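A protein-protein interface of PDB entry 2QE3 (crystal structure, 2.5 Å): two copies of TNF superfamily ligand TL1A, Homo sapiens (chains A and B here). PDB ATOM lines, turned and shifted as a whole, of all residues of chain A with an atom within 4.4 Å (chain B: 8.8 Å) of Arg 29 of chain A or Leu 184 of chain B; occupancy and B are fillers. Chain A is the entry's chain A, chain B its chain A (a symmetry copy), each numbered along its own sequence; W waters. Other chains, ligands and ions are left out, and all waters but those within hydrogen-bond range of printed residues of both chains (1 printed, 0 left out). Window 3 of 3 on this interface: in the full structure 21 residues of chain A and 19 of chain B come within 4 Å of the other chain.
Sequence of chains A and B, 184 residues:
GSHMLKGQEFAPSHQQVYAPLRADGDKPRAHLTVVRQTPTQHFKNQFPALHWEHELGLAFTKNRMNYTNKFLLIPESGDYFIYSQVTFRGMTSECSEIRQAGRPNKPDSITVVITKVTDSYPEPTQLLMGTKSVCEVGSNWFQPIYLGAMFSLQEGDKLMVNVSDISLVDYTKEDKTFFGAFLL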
ATOM      1  N   GLY A  25       5.077  32.052   7.115  1.00  0.00           N
ATOM      2  CA  GLY A  25       4.118  32.070   8.201  1.00  0.00           C
ATOM      3  C   GLY A  25       3.897  30.643   8.629  1.00  0.00           C
ATOM      4  O   GLY A  25       3.252  29.941   7.901  1.00  0.00           O
ATOM      5  N   LYS A  27       3.113  32.356  11.123  1.00  0.00           N
ATOM      6  CA  LYS A  27       2.166  33.177  11.850  1.00  0.00           C
ATOM      7  C   LYS A  27       1.471  32.351  12.952  1.00  0.00           C
ATOM      8  O   LYS A  27       1.157  31.197  12.716  1.00  0.00           O
ATOM      9  CB  LYS A  27       1.114  33.668  10.846  1.00  0.00           C
ATOM     10  CG  LYS A  27       1.512  34.865   9.998  1.00  0.00           C
ATOM     11  CD  LYS A  27       0.636  34.977   8.727  1.00  0.00           C
ATOM     12  CE  LYS A  27       1.159  36.062   7.757  1.00  0.00           C
ATOM     13  NZ  LYS A  27       0.554  37.391   8.064  1.00  0.00           N
ATOM     14  N   PRO A  28       1.190  32.930  14.137  1.00  0.00           N
ATOM     15  CA  PRO A  28       0.507  32.272  15.249  1.00  0.00           C
ATOM     16  C   PRO A  28      -0.939  31.906  14.980  1.00  0.00           C
ATOM     17  O   PRO A  28      -1.724  32.692  14.456  1.00  0.00           O
ATOM     18  CB  PRO A  28       0.456  33.356  16.306  1.00  0.00           C
ATOM     19  CG  PRO A  28       1.442  34.315  15.948  1.00  0.00           C
ATOM     20  CD  PRO A  28       1.533  34.314  14.483  1.00  0.00           C
ATOM     21  N   ARG A  29      -1.307  30.733  15.429  1.00  0.00           N
ATOM     22  CA  ARG A  29      -2.504  30.125  14.953  1.00  0.00           C
ATOM     23  C   ARG A  29      -2.893  29.069  15.936  1.00  0.00           C
ATOM     24  O   ARG A  29      -2.058  28.294  16.407  1.00  0.00           O
ATOM     25  CB  ARG A  29      -2.173  29.393  13.681  1.00  0.00           C
ATOM     26  CG  ARG A  29      -2.152  30.260  12.469  1.00  0.00           C
ATOM     27  CD  ARG A  29      -1.920  29.495  11.164  1.00  0.00           C
ATOM     28  NE  ARG A  29      -1.690  30.445  10.082  1.00  0.00           N
ATOM     29  CZ  ARG A  29      -1.124  30.114   8.925  1.00  0.00           C
ATOM     30  NH1 ARG A  29      -0.747  28.850   8.730  1.00  0.00           N
ATOM     31  NH2 ARG A  29      -0.937  31.027   7.975  1.00  0.00           N
ATOM     32  N   ALA A  30      -4.181  29.001  16.199  1.00  0.00           N
ATOM     33  CA  ALA A  30      -4.653  28.029  17.139  1.00  0.00           C
ATOM     34  C   ALA A  30      -6.091  27.709  16.904  1.00  0.00           C
ATOM     35  O   ALA A  30      -6.941  28.628  16.719  1.00  0.00           O
ATOM     36  CB  ALA A  30      -4.476  28.537  18.484  1.00  0.00           C
ATOM     37  N   PHE A  60      -5.026  22.373  17.996  1.00  0.00           N
ATOM     38  CA  PHE A  60      -3.601  22.540  17.928  1.00  0.00           C
ATOM     39  C   PHE A  60      -3.270  23.964  18.296  1.00  0.00           C
ATOM     40  O   PHE A  60      -4.088  24.884  18.168  1.00  0.00           O
ATOM     41  CB  PHE A  60      -3.157  22.277  16.503  1.00  0.00           C
ATOM     42  CG  PHE A  60      -3.539  23.406  15.530  1.00  0.00           C
ATOM     43  CD1 PHE A  60      -2.861  24.606  15.522  1.00  0.00           C
ATOM     44  CD2 PHE A  60      -4.603  23.259  14.634  1.00  0.00           C
ATOM     45  CE1 PHE A  60      -3.257  25.638  14.670  1.00  0.00           C
ATOM     46  CE2 PHE A  60      -4.980  24.277  13.752  1.00  0.00           C
ATOM     47  CZ  PHE A  60      -4.314  25.458  13.773  1.00  0.00           C
ATOM     48  N   THR A  61      -2.036  24.175  18.705  1.00  0.00           N
ATOM     49  CA  THR A  61      -1.539  25.547  18.708  1.00  0.00           C
ATOM     50  C   THR A  61      -0.176  25.552  18.038  1.00  0.00           C
ATOM     51  O   THR A  61       0.549  24.573  18.113  1.00  0.00           O
ATOM     52  CB  THR A  61      -1.293  26.006  20.087  1.00  0.00           C
ATOM     53  OG1 THR A  61      -0.455  25.021  20.698  1.00  0.00           O
ATOM     54  CG2 THR A  61      -2.568  26.079  20.845  1.00  0.00           C
ATOM     55  N   LYS A  62       0.194  26.646  17.403  1.00  0.00           N
ATOM     56  CA  LYS A  62       1.479  26.641  16.748  1.00  0.00           C
ATOM     57  C   LYS A  62       2.042  28.049  16.680  1.00  0.00           C
ATOM     58  O   LYS A  62       1.338  29.043  16.952  1.00  0.00           O
ATOM     59  CB  LYS A  62       1.405  25.941  15.372  1.00  0.00           C
ATOM     60  CG  LYS A  62       0.552  26.588  14.362  1.00  0.00           C
ATOM     61  CD  LYS A  62       0.242  25.625  13.227  1.00  0.00           C
ATOM     62  CE  LYS A  62       1.480  25.169  12.423  1.00  0.00           C
ATOM     63  NZ  LYS A  62       1.103  24.304  11.234  1.00  0.00           N
ATOM     64  N   MET A  65       1.913  30.328  20.048  1.00  0.00           N
ATOM     65  CA  MET A  65       0.598  30.598  20.612  1.00  0.00           C
ATOM     66  C   MET A  65       0.582  29.822  21.864  1.00  0.00           C
ATOM     67  O   MET A  65       1.094  28.720  21.884  1.00  0.00           O
ATOM     68  CB  MET A  65      -0.467  30.073  19.687  1.00  0.00           C
ATOM     69  CG  MET A  65      -1.019  31.077  18.683  1.00  0.00           C
ATOM     70  SD  MET A  65      -2.178  32.201  19.544  1.00  0.00           S
ATOM     71  CE  MET A  65      -3.114  32.789  18.172  1.00  0.00           C
ATOM     72  N   ALA A 181      -8.192  31.222  16.724  1.00  0.00           N
ATOM     73  CA  ALA A 181      -7.680  32.530  16.276  1.00  0.00           C
ATOM     74  C   ALA A 181      -6.427  32.444  15.422  1.00  0.00           C
ATOM     75  O   ALA A 181      -5.578  31.517  15.597  1.00  0.00           O
ATOM     76  CB  ALA A 181      -7.372  33.371  17.411  1.00  0.00           C
ATOM     77  N   PHE A 182      -6.316  33.380  14.473  1.00  0.00           N
ATOM     78  CA  PHE A 182      -5.030  33.467  13.792  1.00  0.00           C
ATOM     79  C   PHE A 182      -4.584  34.824  13.491  1.00  0.00           C
ATOM     80  O   PHE A 182      -5.387  35.752  13.393  1.00  0.00           O
ATOM     81  CB  PHE A 182      -5.016  32.741  12.531  1.00  0.00           C
ATOM     82  CG  PHE A 182      -6.301  32.813  11.814  1.00  0.00           C
ATOM     83  CD1 PHE A 182      -6.489  33.731  10.816  1.00  0.00           C
ATOM     84  CD2 PHE A 182      -7.317  31.946  12.106  1.00  0.00           C
ATOM     85  CE1 PHE A 182      -7.698  33.809  10.124  1.00  0.00           C
ATOM     86  CE2 PHE A 182      -8.516  32.009  11.419  1.00  0.00           C
ATOM     87  CZ  PHE A 182      -8.716  32.956  10.421  1.00  0.00           C
ATOM     88  N   ASP B  24       1.388  39.237  -3.084  1.00  0.00           N
ATOM     89  CA  ASP B  24       1.639  37.719  -3.222  1.00  0.00           C
ATOM     90  C   ASP B  24       0.482  36.671  -2.827  1.00  0.00           C
ATOM     91  O   ASP B  24      -0.131  36.724  -1.743  1.00  0.00           O
ATOM     92  CB  ASP B  24       2.972  37.295  -2.538  1.00  0.00           C
ATOM     93  CG  ASP B  24       3.235  35.762  -2.615  1.00  0.00           C
ATOM     94  OD1 ASP B  24       2.847  35.008  -1.674  1.00  0.00           O
ATOM     95  OD2 ASP B  24       3.826  35.312  -3.623  1.00  0.00           O
ATOM     96  N   LYS B  27      -2.406  32.073  -3.478  1.00  0.00           N
ATOM     97  CA  LYS B  27      -2.906  31.103  -2.525  1.00  0.00           C
ATOM     98  C   LYS B  27      -4.253  30.523  -3.002  1.00  0.00           C
ATOM     99  O   LYS B  27      -5.062  31.267  -3.530  1.00  0.00           O
ATOM    100  CB  LYS B  27      -3.111  31.830  -1.189  1.00  0.00           C
ATOM    101  CG  LYS B  27      -1.864  32.030  -0.342  1.00  0.00           C
ATOM    102  CD  LYS B  27      -2.062  33.156   0.700  1.00  0.00           C
ATOM    103  CE  LYS B  27      -0.743  33.510   1.428  1.00  0.00           C
ATOM    104  NZ  LYS B  27      -0.562  32.669   2.647  1.00  0.00           N
ATOM    105  N   PRO B  28      -4.526  29.220  -2.791  1.00  0.00           N
ATOM    106  CA  PRO B  28      -5.774  28.555  -3.162  1.00  0.00           C
ATOM    107  C   PRO B  28      -6.997  29.030  -2.402  1.00  0.00           C
ATOM    108  O   PRO B  28      -6.989  29.184  -1.184  1.00  0.00           O
ATOM    109  CB  PRO B  28      -5.549  27.128  -2.706  1.00  0.00           C
ATOM    110  CG  PRO B  28      -4.144  26.970  -2.558  1.00  0.00           C
ATOM    111  CD  PRO B  28      -3.603  28.273  -2.156  1.00  0.00           C
ATOM    112  N   ARG B  29      -8.079  29.173  -3.126  1.00  0.00           N
ATOM    113  CA  ARG B  29      -9.179  29.929  -2.630  1.00  0.00           C
ATOM    114  C   ARG B  29     -10.384  29.544  -3.426  1.00  0.00           C
ATOM    115  O   ARG B  29     -10.330  29.431  -4.653  1.00  0.00           O
ATOM    116  CB  ARG B  29      -8.925  31.376  -2.951  1.00  0.00           C
ATOM    117  CG  ARG B  29      -8.034  32.068  -1.978  1.00  0.00           C
ATOM    118  CD  ARG B  29      -7.864  33.565  -2.249  1.00  0.00           C
ATOM    119  NE  ARG B  29      -6.808  34.093  -1.393  1.00  0.00           N
ATOM    120  CZ  ARG B  29      -6.188  35.247  -1.623  1.00  0.00           C
ATOM    121  NH1 ARG B  29      -6.543  35.969  -2.685  1.00  0.00           N
ATOM    122  NH2 ARG B  29      -5.228  35.675  -0.806  1.00  0.00           N
ATOM    123  N   MET B  65      -7.333  25.077  -6.937  1.00  0.00           N
ATOM    124  CA  MET B  65      -8.370  24.516  -6.081  1.00  0.00           C
ATOM    125  C   MET B  65      -9.218  23.748  -7.007  1.00  0.00           C
ATOM    126  O   MET B  65      -9.450  24.199  -8.112  1.00  0.00           O
ATOM    127  CB  MET B  65      -9.178  25.628  -5.471  1.00  0.00           C
ATOM    128  CG  MET B  65      -8.715  26.102  -4.097  1.00  0.00           C
ATOM    129  SD  MET B  65      -9.250  24.885  -2.840  1.00  0.00           S
ATOM    130  CE  MET B  65      -9.195  25.891  -1.395  1.00  0.00           C
ATOM    131  N   GLU B  76      -2.670  21.882  -1.637  1.00  0.00           N
ATOM    132  CA  GLU B  76      -1.400  22.287  -1.041  1.00  0.00           C
ATOM    133  C   GLU B  76      -1.623  22.076   0.392  1.00  0.00           C
ATOM    134  O   GLU B  76      -2.665  22.510   0.891  1.00  0.00           O
ATOM    135  CB  GLU B  76      -1.128  23.776  -1.302  1.00  0.00           C
ATOM    136  CG  GLU B  76      -0.061  24.404  -0.344  1.00  0.00           C
ATOM    137  CD  GLU B  76       0.428  25.809  -0.806  1.00  0.00           C
ATOM    138  OE1 GLU B  76      -0.006  26.257  -1.949  1.00  0.00           O
ATOM    139  OE2 GLU B  76       1.237  26.435  -0.012  1.00  0.00           O
ATOM    140  N   SER B  77      -0.691  21.410   1.075  1.00  0.00           N
ATOM    141  CA  SER B  77      -0.902  21.164   2.496  1.00  0.00           C
ATOM    142  C   SER B  77      -0.693  22.491   3.183  1.00  0.00           C
ATOM    143  O   SER B  77       0.179  23.253   2.787  1.00  0.00           O
ATOM    144  CB  SER B  77       0.089  20.158   3.011  1.00  0.00           C
ATOM    145  OG  SER B  77       0.060  18.976   2.260  1.00  0.00           O
ATOM    146  N   GLY B  78      -1.522  22.817   4.171  1.00  0.00           N
ATOM    147  CA  GLY B  78      -1.369  24.091   4.899  1.00  0.00           C
ATOM    148  C   GLY B  78      -2.562  24.347   5.786  1.00  0.00           C
ATOM    149  O   GLY B  78      -3.473  23.498   5.932  1.00  0.00           O
ATOM    150  N   ASP B  79      -2.600  25.534   6.380  1.00  0.00           N
ATOM    151  CA  ASP B  79      -3.762  25.752   7.195  1.00  0.00           C
ATOM    152  C   ASP B  79      -4.758  26.520   6.458  1.00  0.00           C
ATOM    153  O   ASP B  79      -4.397  27.523   5.888  1.00  0.00           O
ATOM    154  CB  ASP B  79      -3.352  26.366   8.486  1.00  0.00           C
ATOM    155  CG  ASP B  79      -2.248  25.582   9.117  1.00  0.00           C
ATOM    156  OD1 ASP B  79      -2.212  24.337   8.886  1.00  0.00           O
ATOM    157  OD2 ASP B  79      -1.385  26.190   9.795  1.00  0.00           O
ATOM    158  N   TYR B  80      -5.990  25.995   6.403  1.00  0.00           N
ATOM    159  CA  TYR B  80      -7.111  26.656   5.693  1.00  0.00           C
ATOM    160  C   TYR B  80      -8.241  27.110   6.595  1.00  0.00           C
ATOM    161  O   TYR B  80      -8.510  26.535   7.642  1.00  0.00           O
ATOM    162  CB  TYR B  80      -7.754  25.760   4.651  1.00  0.00           C
ATOM    163  CG  TYR B  80      -6.863  25.367   3.511  1.00  0.00           C
ATOM    164  CD1 TYR B  80      -6.985  25.972   2.287  1.00  0.00           C
ATOM    165  CD2 TYR B  80      -5.901  24.369   3.670  1.00  0.00           C
ATOM    166  CE1 TYR B  80      -6.179  25.619   1.271  1.00  0.00           C
ATOM    167  CE2 TYR B  80      -5.095  23.995   2.660  1.00  0.00           C
ATOM    168  CZ  TYR B  80      -5.232  24.615   1.451  1.00  0.00           C
ATOM    169  OH  TYR B  80      -4.408  24.240   0.407  1.00  0.00           O
ATOM    170  N   PHE B  81      -8.911  28.175   6.193  1.00  0.00           N
ATOM    171  CA  PHE B  81     -10.054  28.578   6.945  1.00  0.00           C
ATOM    172  C   PHE B  81     -11.148  28.142   6.070  1.00  0.00           C
ATOM    173  O   PHE B  81     -11.101  28.362   4.841  1.00  0.00           O
ATOM    174  CB  PHE B  81     -10.151  30.085   7.146  1.00  0.00           C
ATOM    175  CG  PHE B  81     -11.345  30.468   7.896  1.00  0.00           C
ATOM    176  CD1 PHE B  81     -11.369  30.366   9.256  1.00  0.00           C
ATOM    177  CD2 PHE B  81     -12.511  30.845   7.242  1.00  0.00           C
ATOM    178  CE1 PHE B  81     -12.511  30.685  10.004  1.00  0.00           C
ATOM    179  CE2 PHE B  81     -13.684  31.157   7.990  1.00  0.00           C
ATOM    180  CZ  PHE B  81     -13.663  31.076   9.402  1.00  0.00           C
ATOM    181  N   ILE B  82     -12.143  27.565   6.722  1.00  0.00           N
ATOM    182  CA  ILE B  82     -13.242  26.938   6.022  1.00  0.00           C
ATOM    183  C   ILE B  82     -14.575  27.473   6.471  1.00  0.00           C
ATOM    184  O   ILE B  82     -14.744  27.771   7.666  1.00  0.00           O
ATOM    185  CB  ILE B  82     -13.190  25.473   6.346  1.00  0.00           C
ATOM    186  CG1 ILE B  82     -12.546  24.765   5.215  1.00  0.00           C
ATOM    187  CG2 ILE B  82     -14.466  24.893   6.541  1.00  0.00           C
ATOM    188  CD1 ILE B  82     -11.154  25.092   5.230  1.00  0.00           C
ATOM    189  N   ALA B 149     -14.076  27.513  10.464  1.00  0.00           N
ATOM    190  CA  ALA B 149     -12.918  27.465  11.350  1.00  0.00           C
ATOM    191  C   ALA B 149     -11.686  27.184  10.554  1.00  0.00           C
ATOM    192  O   ALA B 149     -11.734  27.034   9.317  1.00  0.00           O
ATOM    193  CB  ALA B 149     -13.078  26.456  12.378  1.00  0.00           C
ATOM    194  N   MET B 150     -10.571  27.133  11.268  1.00  0.00           N
ATOM    195  CA  MET B 150      -9.299  26.886  10.639  1.00  0.00           C
ATOM    196  C   MET B 150      -8.907  25.397  10.779  1.00  0.00           C
ATOM    197  O   MET B 150      -9.178  24.754  11.788  1.00  0.00           O
ATOM    198  CB  MET B 150      -8.295  27.760  11.330  1.00  0.00           C
ATOM    199  CG  MET B 150      -6.807  27.289  11.289  1.00  0.00           C
ATOM    200  SD  MET B 150      -5.800  28.650  11.969  1.00  0.00           S
ATOM    201  CE  MET B 150      -6.293  28.698  13.684  1.00  0.00           C
ATOM    202  N   PHE B 151      -8.293  24.828   9.751  1.00  0.00           N
ATOM    203  CA  PHE B 151      -7.807  23.474   9.863  1.00  0.00           C
ATOM    204  C   PHE B 151      -6.563  23.281   9.082  1.00  0.00           C
ATOM    205  O   PHE B 151      -6.330  23.955   8.033  1.00  0.00           O
ATOM    206  CB  PHE B 151      -8.818  22.443   9.428  1.00  0.00           C
ATOM    207  CG  PHE B 151     -10.131  22.598  10.097  1.00  0.00           C
ATOM    208  CD1 PHE B 151     -10.401  21.938  11.288  1.00  0.00           C
ATOM    209  CD2 PHE B 151     -11.113  23.433   9.564  1.00  0.00           C
ATOM    210  CE1 PHE B 151     -11.659  22.074  11.924  1.00  0.00           C
ATOM    211  CE2 PHE B 151     -12.369  23.573  10.200  1.00  0.00           C
ATOM    212  CZ  PHE B 151     -12.625  22.882  11.375  1.00  0.00           C
ATOM    213  N   SER B 152      -5.750  22.374   9.615  1.00  0.00           N
ATOM    214  CA  SER B 152      -4.554  21.969   8.954  1.00  0.00           C
ATOM    215  C   SER B 152      -4.899  20.814   8.053  1.00  0.00           C
ATOM    216  O   SER B 152      -5.397  19.792   8.558  1.00  0.00           O
ATOM    217  CB  SER B 152      -3.545  21.565   9.986  1.00  0.00           C
ATOM    218  OG  SER B 152      -3.080  22.741  10.607  1.00  0.00           O
ATOM    219  N   ALA B 181     -13.484  28.133   1.235  1.00  0.00           N
ATOM    220  CA  ALA B 181     -12.218  27.922   1.960  1.00  0.00           C
ATOM    221  C   ALA B 181     -11.033  28.662   1.363  1.00  0.00           C
ATOM    222  O   ALA B 181     -10.958  28.880   0.116  1.00  0.00           O
ATOM    223  CB  ALA B 181     -11.879  26.516   1.990  1.00  0.00           C
ATOM    224  N   PHE B 182     -10.119  29.083   2.245  1.00  0.00           N
ATOM    225  CA  PHE B 182      -8.868  29.589   1.693  1.00  0.00           C
ATOM    226  C   PHE B 182      -7.673  29.227   2.448  1.00  0.00           C
ATOM    227  O   PHE B 182      -7.736  28.938   3.642  1.00  0.00           O
ATOM    228  CB  PHE B 182      -8.857  31.039   1.575  1.00  0.00           C
ATOM    229  CG  PHE B 182      -9.567  31.709   2.679  1.00  0.00           C
ATOM    230  CD1 PHE B 182      -8.876  32.198   3.755  1.00  0.00           C
ATOM    231  CD2 PHE B 182     -10.922  31.887   2.634  1.00  0.00           C
ATOM    232  CE1 PHE B 182      -9.533  32.839   4.805  1.00  0.00           C
ATOM    233  CE2 PHE B 182     -11.581  32.530   3.667  1.00  0.00           C
ATOM    234  CZ  PHE B 182     -10.884  33.006   4.772  1.00  0.00           C
ATOM    235  N   LEU B 183      -6.567  29.221   1.723  1.00  0.00           N
ATOM    236  CA  LEU B 183      -5.339  28.955   2.396  1.00  0.00           C
ATOM    237  C   LEU B 183      -4.945  30.147   3.192  1.00  0.00           C
ATOM    238  O   LEU B 183      -4.928  31.286   2.679  1.00  0.00           O
ATOM    239  CB  LEU B 183      -4.267  28.722   1.395  1.00  0.00           C
ATOM    240  CG  LEU B 183      -3.025  28.229   2.127  1.00  0.00           C
ATOM    241  CD1 LEU B 183      -3.249  26.961   2.971  1.00  0.00           C
ATOM    242  CD2 LEU B 183      -1.929  28.049   1.092  1.00  0.00           C
ATOM    243  N   LEU B 184      -4.591  29.900   4.436  1.00  0.00           N
ATOM    244  CA  LEU B 184      -4.096  30.982   5.280  1.00  0.00           C
ATOM    245  C   LEU B 184      -2.686  31.540   4.995  1.00  0.00           C
ATOM    246  O   LEU B 184      -1.707  30.786   4.713  1.00  0.00           O
ATOM    247  CB  LEU B 184      -4.129  30.540   6.690  1.00  0.00           C
ATOM    248  CG  LEU B 184      -5.559  30.674   7.148  1.00  0.00           C
ATOM    249  CD1 LEU B 184      -5.737  30.145   8.639  1.00  0.00           C
ATOM    250  CD2 LEU B 184      -5.884  32.146   6.981  1.00  0.00           C
ATOM    251  OXT LEU B 184      -2.521  32.792   5.102  1.00  0.00           O
HETATM  252  O   HOH W   1      -0.356  27.787   5.870  1.00  0.00           O
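NH1 of Arg 29 of chain A is in salt-bridge range of OD2 of Asp 79 of chain B, at 2.9 Å. The chain-end carboxylate (O) of Leu 184 of chain B lies within salt-bridge range of the guanidinium group (NH2) of Arg 29 of chain A, at 3.4 Å. The side-chain amino group of Lys 62 of chain A lies within salt-bridge range of the side-chain carboxylate of Asp 79 of chain B (3.4 Å).
N of Lys 62 of chain A lies within hydrogen-bond range of O of Arg 29 of chain A (3.0 Å). The backbone carbonyl oxygen (O) of Ala 30 of chain A lies within hydrogen-bond range of the backbone NH (N) of Ala 181 of chain A, 2.9 Å away. O of Leu 184 of chain B is in salt-bridge range of NZ of Lys 27 of chain B (3.0 Å). The side-chain hydroxyl (OG) of Ser 152 of chain B sits at hydrogen-bond distance from the side-chain carboxylate (OD1) of Asp 79 of chain B (2.5 Å). The backbone NH of Leu 184 of chain B sits at hydrogen-bond distance from the backbone carbonyl oxygen of Asp 79 of chain B, at 2.8 Å. The backbone carbonyl oxygen (O) of Phe 81 of chain B lies within hydrogen-bond range of the backbone NH (N) of Phe 182 of chain B, at 2.9 Å.
CE of Met 150 of chain B touches O of Ala 30 of chain A, 3.1 Å away. Phe 60 of chain A touches Met 150 of chain B. Ser 152 of chain B touches Phe 60 of chain A. Ala 181 of chain A touches Met 150 of chain B (O to CE, 3.5 Å). Phe 182 of chain A touches Phe 81 of chain B (CZ to CD1, 3.9 Å). Met 150 of chain B touches Phe 182 of chain A (SD to CD2, 3.6 Å). Phe 182 of chain A touches Leu 184 of chain B (CE1 to CD2, 3.99 Å).
Of the printed residues of chain B, Arg 29 of chain A touches Asp 79 and Leu 184. No residue of chain B comes within 4 Å of Pro 28 of chain A. Printed residues of chain B within 4 Å of Ala 30 of chain A: Met 150 (3.1 Å). Of the printed residues of chain B, Phe 182 of chain A touches Phe 81, Met 150 and Leu 184. Printed residues of chain A within 4 Å of Phe 81 of chain B: Phe 182. Printed residues of chain B within 4 Å of Phe 60 of chain A: Met 150 and Ser 152. Printed residues of chain A within 4 Å of Met 150 of chain B: Ala 30 (3.1 Å), Phe 60 (3.8 Å), Ala 181 (3.5 Å) and Phe 182 (3.6 Å). Of the printed residues of chain B, Lys 62 of chain A touches Asp 79 (3.4 Å). Lys 27 of chain A touches none of the printed residues of chain B. The nearest printed residue of chain B that does not touch Phe 182 of chain A is Phe 182 of chain B (5.7 Å).
Of the 11 printed residues of chain A, 6 touch a printed residue of chain B. Of the 20 printed residues of chain B, 5 touch a printed residue of chain A. Printed residues of chain B that touch a printed residue of chain A: Asp 79, Phe 81, Met 150, Ser 152 and Leu 184. Hydrophobic or aromatic side chains of chain B within 4 Å of the printed part of chain A: Phe 81, Met 150 and Leu 184.
Positions printed for both chains: 27, 28, 29, 65, 181 and 182. Of the 10 pairs that touch across the chains among the printed residues, none has its exchanged pair printed and touching as well.
Water W1 lies within hydrogen-bond range of NH1 of Arg 29 of chain A (3.1 Å), N of Asp 79 of chain B (3.2 Å) and O of Leu 184 of chain B (3.5 Å).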
